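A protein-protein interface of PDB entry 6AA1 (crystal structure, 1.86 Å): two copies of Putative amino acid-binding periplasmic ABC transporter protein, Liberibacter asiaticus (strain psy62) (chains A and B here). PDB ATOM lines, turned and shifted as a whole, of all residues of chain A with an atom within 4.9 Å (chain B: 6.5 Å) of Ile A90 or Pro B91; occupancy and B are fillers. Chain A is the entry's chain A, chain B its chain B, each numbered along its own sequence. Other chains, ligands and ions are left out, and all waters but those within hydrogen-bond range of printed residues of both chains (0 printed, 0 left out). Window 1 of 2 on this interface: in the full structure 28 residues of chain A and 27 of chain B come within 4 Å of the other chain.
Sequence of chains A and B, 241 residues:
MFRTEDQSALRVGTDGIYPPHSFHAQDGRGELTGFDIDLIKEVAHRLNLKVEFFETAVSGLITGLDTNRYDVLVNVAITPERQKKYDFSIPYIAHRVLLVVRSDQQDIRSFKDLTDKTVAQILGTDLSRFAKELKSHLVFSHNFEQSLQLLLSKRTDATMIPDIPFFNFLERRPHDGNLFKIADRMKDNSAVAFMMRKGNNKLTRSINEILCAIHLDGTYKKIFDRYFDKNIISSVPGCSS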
ATOM      1  N   PHE A  88      -8.212  -6.737   4.043  1.00  0.00           N
ATOM      2  CA  PHE A  88      -8.065  -7.280   5.366  1.00  0.00           C
ATOM      3  C   PHE A  88      -8.597  -8.701   5.402  1.00  0.00           C
ATOM      4  O   PHE A  88      -9.613  -8.987   4.789  1.00  0.00           O
ATOM      5  CB  PHE A  88      -8.814  -6.427   6.413  1.00  0.00           C
ATOM      6  CG  PHE A  88      -8.045  -5.222   6.893  1.00  0.00           C
ATOM      7  CD1 PHE A  88      -6.981  -5.364   7.749  1.00  0.00           C
ATOM      8  CD2 PHE A  88      -8.442  -3.946   6.554  1.00  0.00           C
ATOM      9  CE1 PHE A  88      -6.282  -4.256   8.221  1.00  0.00           C
ATOM     10  CE2 PHE A  88      -7.760  -2.841   7.023  1.00  0.00           C
ATOM     11  CZ  PHE A  88      -6.681  -2.999   7.866  1.00  0.00           C
ATOM     12  N   SER A  89      -7.942  -9.560   6.163  1.00  0.00           N
ATOM     13  CA  SER A  89      -8.607 -10.805   6.562  1.00  0.00           C
ATOM     14  C   SER A  89      -9.753 -10.504   7.485  1.00  0.00           C
ATOM     15  O   SER A  89      -9.887  -9.403   8.015  1.00  0.00           O
ATOM     16  CB  SER A  89      -7.624 -11.752   7.252  1.00  0.00           C
ATOM     17  OG  SER A  89      -7.296 -11.355   8.577  1.00  0.00           O
ATOM     18  N   ILE A  90     -10.590 -11.503   7.708  1.00  0.00           N
ATOM     19  CA  ILE A  90     -11.466 -11.494   8.853  1.00  0.00           C
ATOM     20  C   ILE A  90     -10.635 -11.239  10.138  1.00  0.00           C
ATOM     21  O   ILE A  90      -9.474 -11.649  10.213  1.00  0.00           O
ATOM     22  CB  ILE A  90     -12.192 -12.865   8.928  1.00  0.00           C
ATOM     23  CG1 ILE A  90     -13.364 -12.787   9.836  1.00  0.00           C
ATOM     24  CG2 ILE A  90     -11.252 -13.989   9.406  1.00  0.00           C
ATOM     25  CD1 ILE A  90     -14.255 -14.019   9.724  1.00  0.00           C
ATOM     26  N   PRO A  91     -11.188 -10.545  11.148  1.00  0.00           N
ATOM     27  CA  PRO A  91     -10.413 -10.256  12.363  1.00  0.00           C
ATOM     28  C   PRO A  91     -10.040 -11.497  13.123  1.00  0.00           C
ATOM     29  O   PRO A  91     -10.828 -12.442  13.168  1.00  0.00           O
ATOM     30  CB  PRO A  91     -11.367  -9.422  13.210  1.00  0.00           C
ATOM     31  CG  PRO A  91     -12.222  -8.745  12.184  1.00  0.00           C
ATOM     32  CD  PRO A  91     -12.458  -9.797  11.148  1.00  0.00           C
ATOM     33  N   TYR A  92      -8.842 -11.513  13.688  1.00  0.00           N
ATOM     34  CA  TYR A  92      -8.412 -12.738  14.451  1.00  0.00           C
ATOM     35  C   TYR A  92      -8.099 -12.519  15.941  1.00  0.00           C
ATOM     36  O   TYR A  92      -7.868 -13.466  16.668  1.00  0.00           O
ATOM     37  CB  TYR A  92      -7.253 -13.417  13.711  1.00  0.00           C
ATOM     38  CG  TYR A  92      -5.947 -12.645  13.651  1.00  0.00           C
ATOM     39  CD1 TYR A  92      -5.065 -12.666  14.706  1.00  0.00           C
ATOM     40  CD2 TYR A  92      -5.580 -11.956  12.514  1.00  0.00           C
ATOM     41  CE1 TYR A  92      -3.867 -11.952  14.689  1.00  0.00           C
ATOM     42  CE2 TYR A  92      -4.364 -11.294  12.444  1.00  0.00           C
ATOM     43  CZ  TYR A  92      -3.512 -11.292  13.530  1.00  0.00           C
ATOM     44  OH  TYR A  92      -2.320 -10.628  13.384  1.00  0.00           O
ATOM     45  N   VAL A 192      -8.417  -6.566  14.973  1.00  0.00           N
ATOM     46  CA  VAL A 192      -7.089  -6.739  14.389  1.00  0.00           C
ATOM     47  C   VAL A 192      -7.096  -7.873  13.388  1.00  0.00           C
ATOM     48  O   VAL A 192      -7.787  -8.851  13.606  1.00  0.00           O
ATOM     49  CB  VAL A 192      -6.051  -6.993  15.516  1.00  0.00           C
ATOM     50  CG1 VAL A 192      -4.680  -7.332  14.986  1.00  0.00           C
ATOM     51  CG2 VAL A 192      -5.986  -5.727  16.333  1.00  0.00           C
ATOM     52  N   ALA A 193      -6.482  -7.637  12.233  1.00  0.00           N
ATOM     53  CA  ALA A 193      -6.485  -8.577  11.120  1.00  0.00           C
ATOM     54  C   ALA A 193      -5.164  -8.611  10.381  1.00  0.00           C
ATOM     55  O   ALA A 193      -4.242  -7.797  10.633  1.00  0.00           O
ATOM     56  CB  ALA A 193      -7.601  -8.248  10.138  1.00  0.00           C
ATOM     57  N   ASN A 208      -9.224 -16.545   5.031  1.00  0.00           N
ATOM     58  CA  ASN A 208     -10.445 -16.510   5.845  1.00  0.00           C
ATOM     59  C   ASN A 208     -10.994 -17.904   6.097  1.00  0.00           C
ATOM     60  O   ASN A 208     -11.391 -18.249   7.203  1.00  0.00           O
ATOM     61  CB  ASN A 208     -11.514 -15.593   5.269  1.00  0.00           C
ATOM     62  CG  ASN A 208     -11.135 -14.117   5.369  1.00  0.00           C
ATOM     63  OD1 ASN A 208     -10.086 -13.799   5.955  1.00  0.00           O
ATOM     64  ND2 ASN A 208     -11.967 -13.207   4.787  1.00  0.00           N
ATOM     65  N   LEU A 211      -8.708 -19.614   8.541  1.00  0.00           N
ATOM     66  CA  LEU A 211      -8.885 -19.103   9.891  1.00  0.00           C
ATOM     67  C   LEU A 211     -10.106 -19.733  10.582  1.00  0.00           C
ATOM     68  O   LEU A 211     -10.042 -20.076  11.791  1.00  0.00           O
ATOM     69  CB  LEU A 211      -8.928 -17.596   9.920  1.00  0.00           C
ATOM     70  CG  LEU A 211      -7.548 -16.886   9.845  1.00  0.00           C
ATOM     71  CD1 LEU A 211      -7.781 -15.396   9.655  1.00  0.00           C
ATOM     72  CD2 LEU A 211      -6.690 -17.127  11.053  1.00  0.00           C
ATOM     73  N   ILE B  78     -20.844 -17.393   9.342  1.00  0.00           N
ATOM     74  CA  ILE B  78     -19.642 -17.744   8.575  1.00  0.00           C
ATOM     75  C   ILE B  78     -19.272 -19.216   8.838  1.00  0.00           C
ATOM     76  O   ILE B  78     -19.198 -19.654   9.984  1.00  0.00           O
ATOM     77  CB  ILE B  78     -18.454 -16.795   8.942  1.00  0.00           C
ATOM     78  CG1 ILE B  78     -18.865 -15.309   8.723  1.00  0.00           C
ATOM     79  CG2 ILE B  78     -17.234 -17.129   8.114  1.00  0.00           C
ATOM     80  CD1 ILE B  78     -17.729 -14.299   8.960  1.00  0.00           C
ATOM     81  N   GLN B  83     -17.530 -19.794   2.879  1.00  0.00           N
ATOM     82  CA  GLN B  83     -16.458 -18.856   2.481  1.00  0.00           C
ATOM     83  C   GLN B  83     -15.764 -19.335   1.198  1.00  0.00           C
ATOM     84  O   GLN B  83     -15.173 -18.541   0.477  1.00  0.00           O
ATOM     85  CB  GLN B  83     -15.417 -18.717   3.563  1.00  0.00           C
ATOM     86  CG  GLN B  83     -15.863 -18.173   4.890  1.00  0.00           C
ATOM     87  CD  GLN B  83     -14.762 -18.341   5.962  1.00  0.00           C
ATOM     88  OE1 GLN B  83     -14.351 -19.470   6.230  1.00  0.00           O
ATOM     89  NE2 GLN B  83     -14.286 -17.235   6.558  1.00  0.00           N
ATOM     90  N   SER B  89     -18.942  -9.975   4.364  1.00  0.00           N
ATOM     91  CA  SER B  89     -18.475  -8.812   5.041  1.00  0.00           C
ATOM     92  C   SER B  89     -17.746  -9.202   6.313  1.00  0.00           C
ATOM     93  O   SER B  89     -17.767 -10.360   6.775  1.00  0.00           O
ATOM     94  CB  SER B  89     -19.664  -7.911   5.431  1.00  0.00           C
ATOM     95  OG  SER B  89     -20.409  -8.438   6.554  1.00  0.00           O
ATOM     96  N   ILE B  90     -17.090  -8.216   6.931  1.00  0.00           N
ATOM     97  CA  ILE B  90     -16.536  -8.436   8.253  1.00  0.00           C
ATOM     98  C   ILE B  90     -17.733  -8.708   9.154  1.00  0.00           C
ATOM     99  O   ILE B  90     -18.805  -8.158   8.938  1.00  0.00           O
ATOM    100  CB  ILE B  90     -15.838  -7.229   8.877  1.00  0.00           C
ATOM    101  CG1 ILE B  90     -16.849  -6.135   9.186  1.00  0.00           C
ATOM    102  CG2 ILE B  90     -14.714  -6.735   8.015  1.00  0.00           C
ATOM    103  CD1 ILE B  90     -16.682  -4.920   8.335  1.00  0.00           C
ATOM    104  N   PRO B  91     -17.552  -9.552  10.179  1.00  0.00           N
ATOM    105  CA  PRO B  91     -18.661  -9.923  11.081  1.00  0.00           C
ATOM    106  C   PRO B  91     -19.250  -8.730  11.834  1.00  0.00           C
ATOM    107  O   PRO B  91     -18.538  -7.822  12.230  1.00  0.00           O
ATOM    108  CB  PRO B  91     -17.999 -10.905  12.071  1.00  0.00           C
ATOM    109  CG  PRO B  91     -16.799 -11.419  11.362  1.00  0.00           C
ATOM    110  CD  PRO B  91     -16.304 -10.242  10.586  1.00  0.00           C
ATOM    111  N   TYR B  92     -20.556  -8.704  11.944  1.00  0.00           N
ATOM    112  CA  TYR B  92     -21.255  -7.658  12.702  1.00  0.00           C
ATOM    113  C   TYR B  92     -21.992  -8.033  13.993  1.00  0.00           C
ATOM    114  O   TYR B  92     -22.500  -7.141  14.723  1.00  0.00           O
ATOM    115  CB  TYR B  92     -22.213  -6.934  11.785  1.00  0.00           C
ATOM    116  CG  TYR B  92     -23.404  -7.669  11.218  1.00  0.00           C
ATOM    117  CD1 TYR B  92     -24.580  -7.785  11.945  1.00  0.00           C
ATOM    118  CD2 TYR B  92     -23.397  -8.166   9.900  1.00  0.00           C
ATOM    119  CE1 TYR B  92     -25.664  -8.454  11.433  1.00  0.00           C
ATOM    120  CE2 TYR B  92     -24.521  -8.779   9.355  1.00  0.00           C
ATOM    121  CZ  TYR B  92     -25.641  -8.929  10.125  1.00  0.00           C
ATOM    122  OH  TYR B  92     -26.758  -9.470   9.563  1.00  0.00           O
ATOM    123  N   ILE B  93     -22.143  -9.331  14.249  1.00  0.00           N
ATOM    124  CA  ILE B  93     -22.747  -9.815  15.449  1.00  0.00           C
ATOM    125  C   ILE B  93     -22.253 -11.273  15.642  1.00  0.00           C
ATOM    126  O   ILE B  93     -21.593 -11.799  14.759  1.00  0.00           O
ATOM    127  CB  ILE B  93     -24.289  -9.716  15.322  1.00  0.00           C
ATOM    128  CG1 ILE B  93     -25.055  -9.976  16.612  1.00  0.00           C
ATOM    129  CG2 ILE B  93     -24.780 -10.751  14.390  1.00  0.00           C
ATOM    130  CD1 ILE B  93     -25.137  -8.911  17.639  1.00  0.00           C
ATOM    131  N   ALA B 191     -19.416 -16.204  14.491  1.00  0.00           N
ATOM    132  CA  ALA B 191     -19.487 -14.981  13.721  1.00  0.00           C
ATOM    133  C   ALA B 191     -20.615 -14.950  12.619  1.00  0.00           C
ATOM    134  O   ALA B 191     -20.813 -15.891  11.849  1.00  0.00           O
ATOM    135  CB  ALA B 191     -18.153 -14.722  13.074  1.00  0.00           C
ATOM    136  N   VAL B 192     -21.332 -13.832  12.582  1.00  0.00           N
ATOM    137  CA  VAL B 192     -22.443 -13.623  11.666  1.00  0.00           C
ATOM    138  C   VAL B 192     -22.088 -12.376  10.831  1.00  0.00           C
ATOM    139  O   VAL B 192     -21.571 -11.372  11.388  1.00  0.00           O
ATOM    140  CB  VAL B 192     -23.754 -13.404  12.441  1.00  0.00           C
ATOM    141  CG1 VAL B 192     -24.862 -12.982  11.486  1.00  0.00           C
ATOM    142  CG2 VAL B 192     -24.114 -14.666  13.254  1.00  0.00           C
ATOM    143  N   ALA B 193     -22.279 -12.480   9.529  1.00  0.00           N
ATOM    144  CA  ALA B 193     -21.968 -11.379   8.563  1.00  0.00           C
ATOM    145  C   ALA B 193     -22.991 -11.259   7.444  1.00  0.00           C
ATOM    146  O   ALA B 193     -23.908 -12.056   7.312  1.00  0.00           O
ATOM    147  CB  ALA B 193     -20.593 -11.596   7.978  1.00  0.00           C
ATOM    148  N   PHE B 194     -22.824 -10.238   6.616  1.00  0.00           N
ATOM    149  CA  PHE B 194     -23.557 -10.152   5.355  1.00  0.00           C
ATOM    150  C   PHE B 194     -22.884 -11.057   4.344  1.00  0.00           C
ATOM    151  O   PHE B 194     -21.669 -11.039   4.234  1.00  0.00           O
ATOM    152  CB  PHE B 194     -23.599  -8.702   4.835  1.00  0.00           C
ATOM    153  CG  PHE B 194     -24.358  -7.777   5.741  1.00  0.00           C
ATOM    154  CD1 PHE B 194     -25.684  -7.958   5.951  1.00  0.00           C
ATOM    155  CD2 PHE B 194     -23.715  -6.756   6.443  1.00  0.00           C
ATOM    156  CE1 PHE B 194     -26.383  -7.147   6.845  1.00  0.00           C
ATOM    157  CE2 PHE B 194     -24.411  -5.877   7.272  1.00  0.00           C
ATOM    158  CZ  PHE B 194     -25.765  -6.086   7.494  1.00  0.00           C
ATOM    159  N   ASN B 208     -17.907  -2.921   4.387  1.00  0.00           N
ATOM    160  CA  ASN B 208     -16.932  -3.001   5.456  1.00  0.00           C
ATOM    161  C   ASN B 208     -16.506  -1.637   5.976  1.00  0.00           C
ATOM    162  O   ASN B 208     -16.461  -1.419   7.178  1.00  0.00           O
ATOM    163  CB  ASN B 208     -15.724  -3.798   5.028  1.00  0.00           C
ATOM    164  CG  ASN B 208     -16.018  -5.286   4.883  1.00  0.00           C
ATOM    165  OD1 ASN B 208     -17.096  -5.764   5.268  1.00  0.00           O
ATOM    166  ND2 ASN B 208     -15.048  -6.033   4.337  1.00  0.00           N
ATOM    167  N   LEU B 211     -19.482  -0.297   7.877  1.00  0.00           N
ATOM    168  CA  LEU B 211     -19.601  -0.942   9.189  1.00  0.00           C
ATOM    169  C   LEU B 211     -18.616  -0.377  10.245  1.00  0.00           C
ATOM    170  O   LEU B 211     -18.981  -0.127  11.402  1.00  0.00           O
ATOM    171  CB  LEU B 211     -19.491  -2.467   9.070  1.00  0.00           C
ATOM    172  CG  LEU B 211     -20.775  -3.091   8.489  1.00  0.00           C
ATOM    173  CD1 LEU B 211     -20.510  -4.551   8.181  1.00  0.00           C
ATOM    174  CD2 LEU B 211     -21.956  -3.016   9.429  1.00  0.00           C
ATOM    175  N   HIS B 215     -19.614   1.569  13.793  1.00  0.00           N
ATOM    176  CA  HIS B 215     -19.065   1.298  15.085  1.00  0.00           C
ATOM    177  C   HIS B 215     -18.487   2.622  15.652  1.00  0.00           C
ATOM    178  O   HIS B 215     -18.700   2.964  16.809  1.00  0.00           O
ATOM    179  CB  HIS B 215     -17.914   0.301  15.041  1.00  0.00           C
ATOM    180  CG  HIS B 215     -18.340  -1.130  14.986  1.00  0.00           C
ATOM    181  ND1 HIS B 215     -18.711  -1.835  16.115  1.00  0.00           N
ATOM    182  CD2 HIS B 215     -18.436  -1.999  13.938  1.00  0.00           C
ATOM    183  CE1 HIS B 215     -19.040  -3.067  15.757  1.00  0.00           C
ATOM    184  NE2 HIS B 215     -18.910  -3.183  14.441  1.00  0.00           N
ATOM    185  N   TYR B 220     -23.718   1.769  15.846  1.00  0.00           N
ATOM    186  CA  TYR B 220     -23.800   0.301  16.059  1.00  0.00           C
ATOM    187  C   TYR B 220     -24.414   0.004  17.426  1.00  0.00           C
ATOM    188  O   TYR B 220     -25.391  -0.768  17.545  1.00  0.00           O
ATOM    189  CB  TYR B 220     -22.440  -0.351  15.951  1.00  0.00           C
ATOM    190  CG  TYR B 220     -22.444  -1.829  16.283  1.00  0.00           C
ATOM    191  CD1 TYR B 220     -22.673  -2.757  15.281  1.00  0.00           C
ATOM    192  CD2 TYR B 220     -22.203  -2.286  17.564  1.00  0.00           C
ATOM    193  CE1 TYR B 220     -22.675  -4.110  15.535  1.00  0.00           C
ATOM    194  CE2 TYR B 220     -22.178  -3.641  17.853  1.00  0.00           C
ATOM    195  CZ  TYR B 220     -22.458  -4.567  16.827  1.00  0.00           C
ATOM    196  OH  TYR B 220     -22.447  -5.937  17.071  1.00  0.00           O
ATOM    197  N   VAL B 236     -19.393  -7.836  18.421  1.00  0.00           N
ATOM    198  CA  VAL B 236     -18.062  -8.060  17.855  1.00  0.00           C
ATOM    199  C   VAL B 236     -17.187  -6.862  18.236  1.00  0.00           C
ATOM    200  O   VAL B 236     -17.696  -5.863  18.734  1.00  0.00           O
ATOM    201  CB  VAL B 236     -18.153  -8.191  16.327  1.00  0.00           C
ATOM    202  CG1 VAL B 236     -18.990  -9.426  15.953  1.00  0.00           C
ATOM    203  CG2 VAL B 236     -18.763  -6.948  15.687  1.00  0.00           C
ATOM    204  N   PRO B 237     -15.890  -6.952  17.993  1.00  0.00           N
ATOM    205  CA  PRO B 237     -15.110  -5.757  18.288  1.00  0.00           C
ATOM    206  C   PRO B 237     -15.470  -4.544  17.444  1.00  0.00           C
ATOM    207  O   PRO B 237     -15.924  -4.663  16.294  1.00  0.00           O
ATOM    208  CB  PRO B 237     -13.645  -6.168  17.993  1.00  0.00           C
ATOM    209  CG  PRO B 237     -13.648  -7.614  17.729  1.00  0.00           C
ATOM    210  CD  PRO B 237     -15.072  -8.091  17.574  1.00  0.00           C
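The backbone carbonyl oxygen (O) of Asn A208 is in hydrogen-bond range of the side-chain amide nitrogen (NE2) of Gln B83.
Ile A90 touches Pro B91, but with the chains exchanged Pro A91 does not touch Ile B90 (4.8 Å). Pro A91 touches its own counterpart, Pro B91. Of the 4 pairs that touch across the chains among the printed residues, 1 has its exchanged pair printed and touching as well.
OD1 of Asn A208 lies within hydrogen-bond range of N of Ile A90, 2.9 Å away. O of Ala B191 is in hydrogen-bond range of N of Ile B78 (2.9 Å).
Ile A90 touches Ile B78. CG1 of Ile A90 touches CD of Pro B91 (3.96 Å). Pro A91 touches Pro B91 (CD to CD, 3.9 Å).
Of the 9 printed residues of chain A, 3 touch a printed residue of chain B. Of the 17 printed residues of chain B, 3 touch a printed residue of chain A. Printed residues of chain B that touch a printed residue of chain A: Ile B78, Gln B83 and Pro B91. Hydrophobic or aromatic side chains of chain B within 4 Å of the printed part of chain A: Ile B78 and Pro B91.
Ile A90 touches just these residues of chain B: Ile B78 (3.6 Å) and Pro B91 (3.96 Å). Of the printed residues of chain B, Asn A208 touches Gln B83 (3.1 Å). Of the printed residues of chain A, Ile B78 touches Ile A90 (3.6 Å). Pro B91 touches just these residues of chain A: Ile A90 (3.96 Å) and Pro A91 (3.9 Å). Ala B193 touches none of the printed residues of chain A. The nearest residue of chain B that does not touch Ile A90 is Gln B83 (4.5 Å). The nearest printed residue of chain A that does not touch Pro B91 is Ser A89 (7.0 Å).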
